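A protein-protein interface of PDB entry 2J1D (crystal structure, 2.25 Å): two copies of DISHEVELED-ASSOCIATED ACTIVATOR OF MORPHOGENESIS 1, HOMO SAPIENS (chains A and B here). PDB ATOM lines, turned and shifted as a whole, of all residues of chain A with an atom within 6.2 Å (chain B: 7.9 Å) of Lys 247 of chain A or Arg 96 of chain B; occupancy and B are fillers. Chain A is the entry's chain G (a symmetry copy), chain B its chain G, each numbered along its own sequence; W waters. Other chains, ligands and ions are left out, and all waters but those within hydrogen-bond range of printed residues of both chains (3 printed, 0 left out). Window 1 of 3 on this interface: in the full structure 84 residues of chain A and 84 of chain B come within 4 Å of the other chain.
Printed residues of chain B within 4 Å of Ser 244 of chain A: Phe 18 (3.4 Å), Trp 20 (3.5 Å) and Ser 21 (2.7 Å). Of the printed residues of chain B, Asn 246 of chain A touches Arg 96. Lys 247 of chain A touches three residues of chain B. Printed residues of chain B within 4 Å of Lys 252 of chain A: Gly 95 (3.7 Å). Of the printed residues of chain A, Ser 21 of chain B touches Ser 244 (2.7 Å). Of chain A, only Asn 246 (3.8 Å), Lys 247 (3.3 Å) and Asp 250 (3.0 Å) come within 4 Å of Arg 96 of chain B. The nearest residue of chain B that does not touch Lys 247 of chain A is Trp 20 of chain B (5.0 Å). The nearest residue of chain A that does not touch Arg 96 of chain B is Lys 252 of chain A (4.4 Å). The nearest printed residue of chain A that does not touch Ser 21 of chain B is Ser 243 of chain A (4.5 Å).
No position is printed for both chains. Of the 14 pairs that touch across the chains among the printed residues, none has its exchanged pair printed and touching as well.
O of Ser 17 of chain B is in hydrogen-bond range of OG1 of Thr 251 of chain A (2.5 Å). The backbone NH (N) of Ser 21 of chain B lies within hydrogen-bond range of the side-chain hydroxyl (OG) of Ser 244 of chain A. The backbone NH (N) of Gly 95 of chain B sits at hydrogen-bond distance from the backbone carbonyl oxygen (O) of Asp 250 of chain A (2.7 Å). The side-chain carboxylate (OD2) of Asp 250 of chain A lies within salt-bridge range of the guanidinium group (NH1) of Arg 96 of chain B, at 3.3 Å. The guanidinium group (NH1) of Arg 96 of chain B lies close to the side-chain amino group (NZ) of Lys 247 of chain A.
The side-chain carboxylate (OD1) of Asp 94 of chain B sits at hydrogen-bond distance from the backbone NH (N) of Arg 96 of chain B (3.0 Å). The guanidinium group (NH1) of Arg 97 of chain B lies within salt-bridge range of the side-chain carboxylate (OD2) of Asp 94 of chain B, 2.9 Å away. ND2 of Asn 100 of chain B lies close to O of Arg 96 of chain B (3.4 Å). The backbone carbonyl oxygen (O) of Ala 249 of chain A lies within hydrogen-bond range of the side-chain amino group (NZ) of Lys 252 of chain A (2.5 Å).
Along chain B the printed residues that touch a printed residue of chain A span positions 17 to 96. Among the printed residues, Asp or Glu carboxylates within 4 Å of a Lys or Arg side-chain nitrogen of the other chain: Asp 250 of chain A with Arg 96 of chain B.
Phe 18 of chain B touches Ser 244 of chain A. Trp 20 of chain B touches Ser 244 of chain A (CA to OG, 3.5 Å). Arg 96 of chain B touches Asn 246 of chain A. Phe 18 of chain B touches Lys 247 of chain A. Asn 19 of chain B touches Lys 247 of chain A. Phe 18 of chain B touches Ile 248 of chain A (CE1 to CG1, 3.5 Å). Asp 250 of chain A touches Asp 94 of chain B. Thr 251 of chain A touches Phe 18 of chain B (OG1 to CA, 3.5 Å). Gly 95 of chain B touches Lys 252 of chain A (CA to CG, 3.7 Å).
Water W3 lies within hydrogen-bond range of OD2 of Asp 94 of chain B (2.5 Å), OD2 of Asp 250 of chain A (2.6 Å) and ND2 of Asn 19 of chain B (2.7 Å). Water W1 lies within hydrogen-bond range of the backbone carbonyl oxygen (O) of Lys 247 of chain A (2.6 Å), the backbone NH (N) of Asn 19 of chain B (2.8 Å) and the side-chain hydroxyl (OG1) of Thr 251 of chain A (3.0 Å). Water W2 bridges the backbone NH of Lys 252 of chain A and the backbone NH of Gly 95 of chain B.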
ATOM      1  N   SER A 243      13.314  38.067  21.006  1.00  0.00           N
ATOM      2  CA  SER A 243      14.043  37.208  20.061  1.00  0.00           C
ATOM      3  C   SER A 243      13.211  36.006  19.593  1.00  0.00           C
ATOM      4  O   SER A 243      13.467  35.452  18.519  1.00  0.00           O
ATOM      5  CB  SER A 243      15.352  36.720  20.676  1.00  0.00           C
ATOM      6  OG  SER A 243      15.116  35.884  21.803  1.00  0.00           O
ATOM      7  N   SER A 244      12.228  35.618  20.414  1.00  0.00           N
ATOM      8  CA  SER A 244      11.286  34.534  20.112  1.00  0.00           C
ATOM      9  C   SER A 244      10.524  34.774  18.823  1.00  0.00           C
ATOM     10  O   SER A 244      10.134  33.828  18.151  1.00  0.00           O
ATOM     11  CB  SER A 244      10.271  34.373  21.240  1.00  0.00           C
ATOM     12  OG  SER A 244      10.906  34.169  22.485  1.00  0.00           O
ATOM     13  N   LEU A 245      10.304  36.045  18.494  1.00  0.00           N
ATOM     14  CA  LEU A 245       9.658  36.430  17.240  1.00  0.00           C
ATOM     15  C   LEU A 245      10.375  35.811  16.062  1.00  0.00           C
ATOM     16  O   LEU A 245       9.751  35.385  15.096  1.00  0.00           O
ATOM     17  CB  LEU A 245       9.657  37.949  17.065  1.00  0.00           C
ATOM     18  CG  LEU A 245       8.750  38.803  17.947  1.00  0.00           C
ATOM     19  CD1 LEU A 245       9.022  40.278  17.639  1.00  0.00           C
ATOM     20  CD2 LEU A 245       7.294  38.443  17.730  1.00  0.00           C
ATOM     21  N   ASN A 246      11.695  35.752  16.160  1.00  0.00           N
ATOM     22  CA  ASN A 246      12.512  35.224  15.070  1.00  0.00           C
ATOM     23  C   ASN A 246      12.617  33.692  15.022  1.00  0.00           C
ATOM     24  O   ASN A 246      13.328  33.143  14.180  1.00  0.00           O
ATOM     25  CB  ASN A 246      13.860  35.928  15.077  1.00  0.00           C
ATOM     26  CG  ASN A 246      13.743  37.340  14.534  1.00  0.00           C
ATOM     27  OD1 ASN A 246      13.170  37.532  13.457  1.00  0.00           O
ATOM     28  ND2 ASN A 246      14.239  38.332  15.279  1.00  0.00           N
ATOM     29  N   LYS A 247      11.844  33.037  15.891  1.00  0.00           N
ATOM     30  CA  LYS A 247      11.699  31.583  15.949  1.00  0.00           C
ATOM     31  C   LYS A 247      10.322  31.110  15.494  1.00  0.00           C
ATOM     32  O   LYS A 247      10.072  29.919  15.466  1.00  0.00           O
ATOM     33  CB  LYS A 247      11.871  31.094  17.396  1.00  0.00           C
ATOM     34  CG  LYS A 247      13.198  31.380  18.032  1.00  0.00           C
ATOM     35  CD  LYS A 247      14.340  30.679  17.304  1.00  0.00           C
ATOM     36  CE  LYS A 247      15.696  31.057  17.896  1.00  0.00           C
ATOM     37  NZ  LYS A 247      16.841  30.839  16.939  1.00  0.00           N
ATOM     38  N   ILE A 248       9.410  32.024  15.177  1.00  0.00           N
ATOM     39  CA  ILE A 248       8.040  31.624  14.820  1.00  0.00           C
ATOM     40  C   ILE A 248       8.041  30.791  13.526  1.00  0.00           C
ATOM     41  O   ILE A 248       7.347  29.776  13.427  1.00  0.00           O
ATOM     42  CB  ILE A 248       7.082  32.839  14.637  1.00  0.00           C
ATOM     43  CG1 ILE A 248       7.089  33.739  15.875  1.00  0.00           C
ATOM     44  CG2 ILE A 248       5.647  32.355  14.363  1.00  0.00           C
ATOM     45  CD1 ILE A 248       6.262  34.974  15.738  1.00  0.00           C
ATOM     46  N   ALA A 249       8.838  31.236  12.554  1.00  0.00           N
ATOM     47  CA  ALA A 249       8.878  30.641  11.227  1.00  0.00           C
ATOM     48  C   ALA A 249       9.582  29.304  11.270  1.00  0.00           C
ATOM     49  O   ALA A 249       9.532  28.540  10.309  1.00  0.00           O
ATOM     50  CB  ALA A 249       9.578  31.577  10.257  1.00  0.00           C
ATOM     51  N   ASP A 250      10.264  29.033  12.378  1.00  0.00           N
ATOM     52  CA  ASP A 250      10.916  27.744  12.592  1.00  0.00           C
ATOM     53  C   ASP A 250       9.953  26.582  12.799  1.00  0.00           C
ATOM     54  O   ASP A 250      10.291  25.450  12.470  1.00  0.00           O
ATOM     55  CB  ASP A 250      11.839  27.811  13.797  1.00  0.00           C
ATOM     56  CG  ASP A 250      13.076  28.652  13.553  1.00  0.00           C
ATOM     57  OD1 ASP A 250      13.267  29.219  12.450  1.00  0.00           O
ATOM     58  OD2 ASP A 250      13.863  28.735  14.503  1.00  0.00           O
ATOM     59  N   THR A 251       8.783  26.856  13.377  1.00  0.00           N
ATOM     60  CA  THR A 251       7.697  25.876  13.464  1.00  0.00           C
ATOM     61  C   THR A 251       7.019  25.680  12.100  1.00  0.00           C
ATOM     62  O   THR A 251       6.542  26.631  11.487  1.00  0.00           O
ATOM     63  CB  THR A 251       6.645  26.305  14.494  1.00  0.00           C
ATOM     64  OG1 THR A 251       7.243  26.353  15.794  1.00  0.00           O
ATOM     65  CG2 THR A 251       5.449  25.335  14.498  1.00  0.00           C
ATOM     66  N   LYS A 252       6.965  24.434  11.649  1.00  0.00           N
ATOM     67  CA  LYS A 252       6.536  24.100  10.292  1.00  0.00           C
ATOM     68  C   LYS A 252       5.196  23.396  10.318  1.00  0.00           C
ATOM     69  O   LYS A 252       4.923  22.621  11.222  1.00  0.00           O
ATOM     70  CB  LYS A 252       7.553  23.167   9.631  1.00  0.00           C
ATOM     71  CG  LYS A 252       8.987  23.636   9.709  1.00  0.00           C
ATOM     72  CD  LYS A 252       9.205  24.930   8.936  1.00  0.00           C
ATOM     73  CE  LYS A 252      10.602  25.501   9.188  1.00  0.00           C
ATOM     74  NZ  LYS A 252      10.690  26.919   8.752  1.00  0.00           N
ATOM     75  N   SER B  17       5.607  22.439  18.550  1.00  0.00           N
ATOM     76  CA  SER B  17       6.027  23.479  19.497  1.00  0.00           C
ATOM     77  C   SER B  17       6.435  24.784  18.825  1.00  0.00           C
ATOM     78  O   SER B  17       6.856  24.805  17.663  1.00  0.00           O
ATOM     79  CB  SER B  17       7.158  22.974  20.394  1.00  0.00           C
ATOM     80  OG  SER B  17       8.352  22.763  19.671  1.00  0.00           O
ATOM     81  N   PHE B  18       6.278  25.871  19.575  1.00  0.00           N
ATOM     82  CA  PHE B  18       6.855  27.167  19.224  1.00  0.00           C
ATOM     83  C   PHE B  18       8.108  27.368  20.098  1.00  0.00           C
ATOM     84  O   PHE B  18       8.033  27.375  21.325  1.00  0.00           O
ATOM     85  CB  PHE B  18       5.799  28.279  19.394  1.00  0.00           C
ATOM     86  CG  PHE B  18       6.334  29.681  19.300  1.00  0.00           C
ATOM     87  CD1 PHE B  18       7.345  30.019  18.409  1.00  0.00           C
ATOM     88  CD2 PHE B  18       5.772  30.689  20.075  1.00  0.00           C
ATOM     89  CE1 PHE B  18       7.806  31.305  18.336  1.00  0.00           C
ATOM     90  CE2 PHE B  18       6.232  31.982  19.999  1.00  0.00           C
ATOM     91  CZ  PHE B  18       7.245  32.291  19.133  1.00  0.00           C
ATOM     92  N   ASN B  19       9.256  27.504  19.446  1.00  0.00           N
ATOM     93  CA  ASN B  19      10.525  27.616  20.146  1.00  0.00           C
ATOM     94  C   ASN B  19      10.769  29.003  20.732  1.00  0.00           C
ATOM     95  O   ASN B  19      11.713  29.696  20.349  1.00  0.00           O
ATOM     96  CB  ASN B  19      11.677  27.228  19.214  1.00  0.00           C
ATOM     97  CG  ASN B  19      13.012  27.142  19.933  1.00  0.00           C
ATOM     98  OD1 ASN B  19      13.094  26.702  21.086  1.00  0.00           O
ATOM     99  ND2 ASN B  19      14.065  27.569  19.253  1.00  0.00           N
ATOM    100  N   TRP B  20       9.939  29.399  21.688  1.00  0.00           N
ATOM    101  CA  TRP B  20      10.054  30.743  22.260  1.00  0.00           C
ATOM    102  C   TRP B  20      10.986  30.721  23.453  1.00  0.00           C
ATOM    103  O   TRP B  20      11.425  29.670  23.854  1.00  0.00           O
ATOM    104  CB  TRP B  20       8.688  31.323  22.635  1.00  0.00           C
ATOM    105  CG  TRP B  20       7.858  30.564  23.645  1.00  0.00           C
ATOM    106  CD1 TRP B  20       8.223  29.468  24.400  1.00  0.00           C
ATOM    107  CD2 TRP B  20       6.523  30.880  24.032  1.00  0.00           C
ATOM    108  NE1 TRP B  20       7.187  29.092  25.212  1.00  0.00           N
ATOM    109  CE2 TRP B  20       6.137  29.945  25.017  1.00  0.00           C
ATOM    110  CE3 TRP B  20       5.612  31.866  23.642  1.00  0.00           C
ATOM    111  CZ2 TRP B  20       4.877  29.969  25.609  1.00  0.00           C
ATOM    112  CZ3 TRP B  20       4.360  31.888  24.230  1.00  0.00           C
ATOM    113  CH2 TRP B  20       4.001  30.948  25.197  1.00  0.00           C
ATOM    114  N   SER B  21      11.320  31.900  23.973  1.00  0.00           N
ATOM    115  CA  SER B  21      11.985  32.037  25.262  1.00  0.00           C
ATOM    116  C   SER B  21      11.083  32.871  26.154  1.00  0.00           C
ATOM    117  O   SER B  21      10.855  34.041  25.885  1.00  0.00           O
ATOM    118  CB  SER B  21      13.340  32.719  25.104  1.00  0.00           C
ATOM    119  OG  SER B  21      14.063  32.160  24.025  1.00  0.00           O
ATOM    120  N   ILE B  93       9.703  19.205  18.096  1.00  0.00           N
ATOM    121  CA  ILE B  93      10.861  20.119  17.916  1.00  0.00           C
ATOM    122  C   ILE B  93      10.734  20.923  16.603  1.00  0.00           C
ATOM    123  O   ILE B  93      10.334  20.368  15.583  1.00  0.00           O
ATOM    124  CB  ILE B  93      12.198  19.295  17.883  1.00  0.00           C
ATOM    125  CG1 ILE B  93      12.557  18.687  19.259  1.00  0.00           C
ATOM    126  CG2 ILE B  93      13.335  20.107  17.331  1.00  0.00           C
ATOM    127  CD1 ILE B  93      12.411  19.602  20.474  1.00  0.00           C
ATOM    128  N   ASP B  94      11.075  22.216  16.619  1.00  0.00           N
ATOM    129  CA  ASP B  94      10.887  23.065  15.413  1.00  0.00           C
ATOM    130  C   ASP B  94      11.712  22.582  14.213  1.00  0.00           C
ATOM    131  O   ASP B  94      12.697  21.858  14.368  1.00  0.00           O
ATOM    132  CB  ASP B  94      11.184  24.535  15.697  1.00  0.00           C
ATOM    133  CG  ASP B  94      12.671  24.833  15.810  1.00  0.00           C
ATOM    134  OD1 ASP B  94      13.386  24.900  14.790  1.00  0.00           O
ATOM    135  OD2 ASP B  94      13.120  25.034  16.940  1.00  0.00           O
ATOM    136  N   GLY B  95      11.302  22.999  13.023  1.00  0.00           N
ATOM    137  CA  GLY B  95      11.856  22.467  11.785  1.00  0.00           C
ATOM    138  C   GLY B  95      13.297  22.856  11.531  1.00  0.00           C
ATOM    139  O   GLY B  95      14.067  22.073  10.974  1.00  0.00           O
ATOM    140  N   ARG B  96      13.657  24.067  11.939  1.00  0.00           N
ATOM    141  CA  ARG B  96      15.019  24.574  11.800  1.00  0.00           C
ATOM    142  C   ARG B  96      15.984  23.742  12.628  1.00  0.00           C
ATOM    143  O   ARG B  96      16.958  23.207  12.109  1.00  0.00           O
ATOM    144  CB  ARG B  96      15.065  26.027  12.254  1.00  0.00           C
ATOM    145  CG  ARG B  96      16.437  26.703  12.284  1.00  0.00           C
ATOM    146  CD  ARG B  96      16.222  28.117  12.794  1.00  0.00           C
ATOM    147  NE  ARG B  96      17.363  29.015  12.670  1.00  0.00           N
ATOM    148  CZ  ARG B  96      17.366  30.281  13.098  1.00  0.00           C
ATOM    149  NH1 ARG B  96      16.276  30.804  13.679  1.00  0.00           N
ATOM    150  NH2 ARG B  96      18.459  31.035  12.943  1.00  0.00           N
ATOM    151  N   ARG B  97      15.703  23.644  13.920  1.00  0.00           N
ATOM    152  CA  ARG B  97      16.529  22.851  14.813  1.00  0.00           C
ATOM    153  C   ARG B  97      16.550  21.377  14.414  1.00  0.00           C
ATOM    154  O   ARG B  97      17.616  20.761  14.387  1.00  0.00           O
ATOM    155  CB  ARG B  97      16.117  23.065  16.275  1.00  0.00           C
ATOM    156  CG  ARG B  97      16.720  24.383  16.805  1.00  0.00           C
ATOM    157  CD  ARG B  97      16.069  24.935  18.069  1.00  0.00           C
ATOM    158  NE  ARG B  97      16.162  23.994  19.179  1.00  0.00           N
ATOM    159  CZ  ARG B  97      15.142  23.360  19.749  1.00  0.00           C
ATOM    160  NH1 ARG B  97      13.882  23.525  19.346  1.00  0.00           N
ATOM    161  NH2 ARG B  97      15.395  22.533  20.743  1.00  0.00           N
ATOM    162  N   ALA B  98      15.388  20.842  14.052  1.00  0.00           N
ATOM    163  CA  ALA B  98      15.274  19.469  13.560  1.00  0.00           C
ATOM    164  C   ALA B  98      16.130  19.218  12.315  1.00  0.00           C
ATOM    165  O   ALA B  98      16.864  18.241  12.271  1.00  0.00           O
ATOM    166  CB  ALA B  98      13.820  19.122  13.279  1.00  0.00           C
ATOM    167  N   GLN B  99      16.046  20.084  11.306  1.00  0.00           N
ATOM    168  CA  GLN B  99      16.882  19.926  10.107  1.00  0.00           C
ATOM    169  C   GLN B  99      18.379  20.038  10.416  1.00  0.00           C
ATOM    170  O   GLN B  99      19.183  19.360   9.792  1.00  0.00           O
ATOM    171  CB  GLN B  99      16.512  20.934   9.007  1.00  0.00           C
ATOM    172  CG  GLN B  99      17.183  20.658   7.622  1.00  0.00           C
ATOM    173  CD  GLN B  99      16.958  19.213   7.087  1.00  0.00           C
ATOM    174  OE1 GLN B  99      15.830  18.692   7.092  1.00  0.00           O
ATOM    175  NE2 GLN B  99      18.037  18.574   6.626  1.00  0.00           N
ATOM    176  N   ASN B 100      18.754  20.911  11.352  1.00  0.00           N
ATOM    177  CA  ASN B 100      20.156  21.032  11.775  1.00  0.00           C
ATOM    178  C   ASN B 100      20.693  19.732  12.351  1.00  0.00           C
ATOM    179  O   ASN B 100      21.848  19.401  12.121  1.00  0.00           O
ATOM    180  CB  ASN B 100      20.343  22.111  12.840  1.00  0.00           C
ATOM    181  CG  ASN B 100      20.193  23.509  12.306  1.00  0.00           C
ATOM    182  OD1 ASN B 100      20.292  23.753  11.096  1.00  0.00           O
ATOM    183  ND2 ASN B 100      19.958  24.457  13.221  1.00  0.00           N
ATOM    184  N   CYS B 101      19.855  19.047  13.134  1.00  0.00           N
ATOM    185  CA  CYS B 101      20.158  17.726  13.694  1.00  0.00           C
ATOM    186  C   CYS B 101      20.325  16.695  12.605  1.00  0.00           C
ATOM    187  O   CYS B 101      21.277  15.921  12.625  1.00  0.00           O
ATOM    188  CB  CYS B 101      19.015  17.206  14.589  1.00  0.00           C
ATOM    189  SG  CYS B 101      18.932  17.852  16.252  1.00  0.00           S
ATOM    190  N   ASN B 102      19.358  16.648  11.689  1.00  0.00           N
ATOM    191  CA  ASN B 102      19.371  15.655  10.626  1.00  0.00           C
ATOM    192  C   ASN B 102      20.622  15.769   9.748  1.00  0.00           C
ATOM    193  O   ASN B 102      21.135  14.758   9.262  1.00  0.00           O
ATOM    194  CB  ASN B 102      18.091  15.741   9.796  1.00  0.00           C
ATOM    195  CG  ASN B 102      16.850  15.298  10.571  1.00  0.00           C
ATOM    196  OD1 ASN B 102      15.749  15.786  10.329  1.00  0.00           O
ATOM    197  ND2 ASN B 102      17.026  14.376  11.499  1.00  0.00           N
ATOM    198  N   ILE B 103      21.125  16.990   9.579  1.00  0.00           N
ATOM    199  CA  ILE B 103      22.397  17.218   8.896  1.00  0.00           C
ATOM    200  C   ILE B 103      23.565  16.600   9.681  1.00  0.00           C
ATOM    201  O   ILE B 103      24.381  15.870   9.118  1.00  0.00           O
ATOM    202  CB  ILE B 103      22.636  18.726   8.668  1.00  0.00           C
ATOM    203  CG1 ILE B 103      21.665  19.252   7.612  1.00  0.00           C
ATOM    204  CG2 ILE B 103      24.066  18.996   8.216  1.00  0.00           C
ATOM    205  CD1 ILE B 103      21.700  20.762   7.447  1.00  0.00           C
ATOM    206  N   PHE B 139      24.027  20.978  19.610  1.00  0.00           N
ATOM    207  CA  PHE B 139      22.692  20.369  19.647  1.00  0.00           C
ATOM    208  C   PHE B 139      22.474  19.541  20.920  1.00  0.00           C
ATOM    209  O   PHE B 139      22.049  18.391  20.863  1.00  0.00           O
ATOM    210  CB  PHE B 139      22.451  19.551  18.373  1.00  0.00           C
ATOM    211  CG  PHE B 139      22.748  20.322  17.123  1.00  0.00           C
ATOM    212  CD1 PHE B 139      23.859  20.028  16.354  1.00  0.00           C
ATOM    213  CD2 PHE B 139      21.950  21.384  16.747  1.00  0.00           C
ATOM    214  CE1 PHE B 139      24.163  20.761  15.217  1.00  0.00           C
ATOM    215  CE2 PHE B 139      22.257  22.132  15.604  1.00  0.00           C
ATOM    216  CZ  PHE B 139      23.368  21.809  14.842  1.00  0.00           C
HETATM  217  O   HOH W   1       9.792  27.630  16.750  1.00  0.00           O
HETATM  218  O   HOH W   2       8.126  22.603  13.346  1.00  0.00           O
HETATM  219  O   HOH W   3      14.244  27.293  16.594  1.00  0.00           O
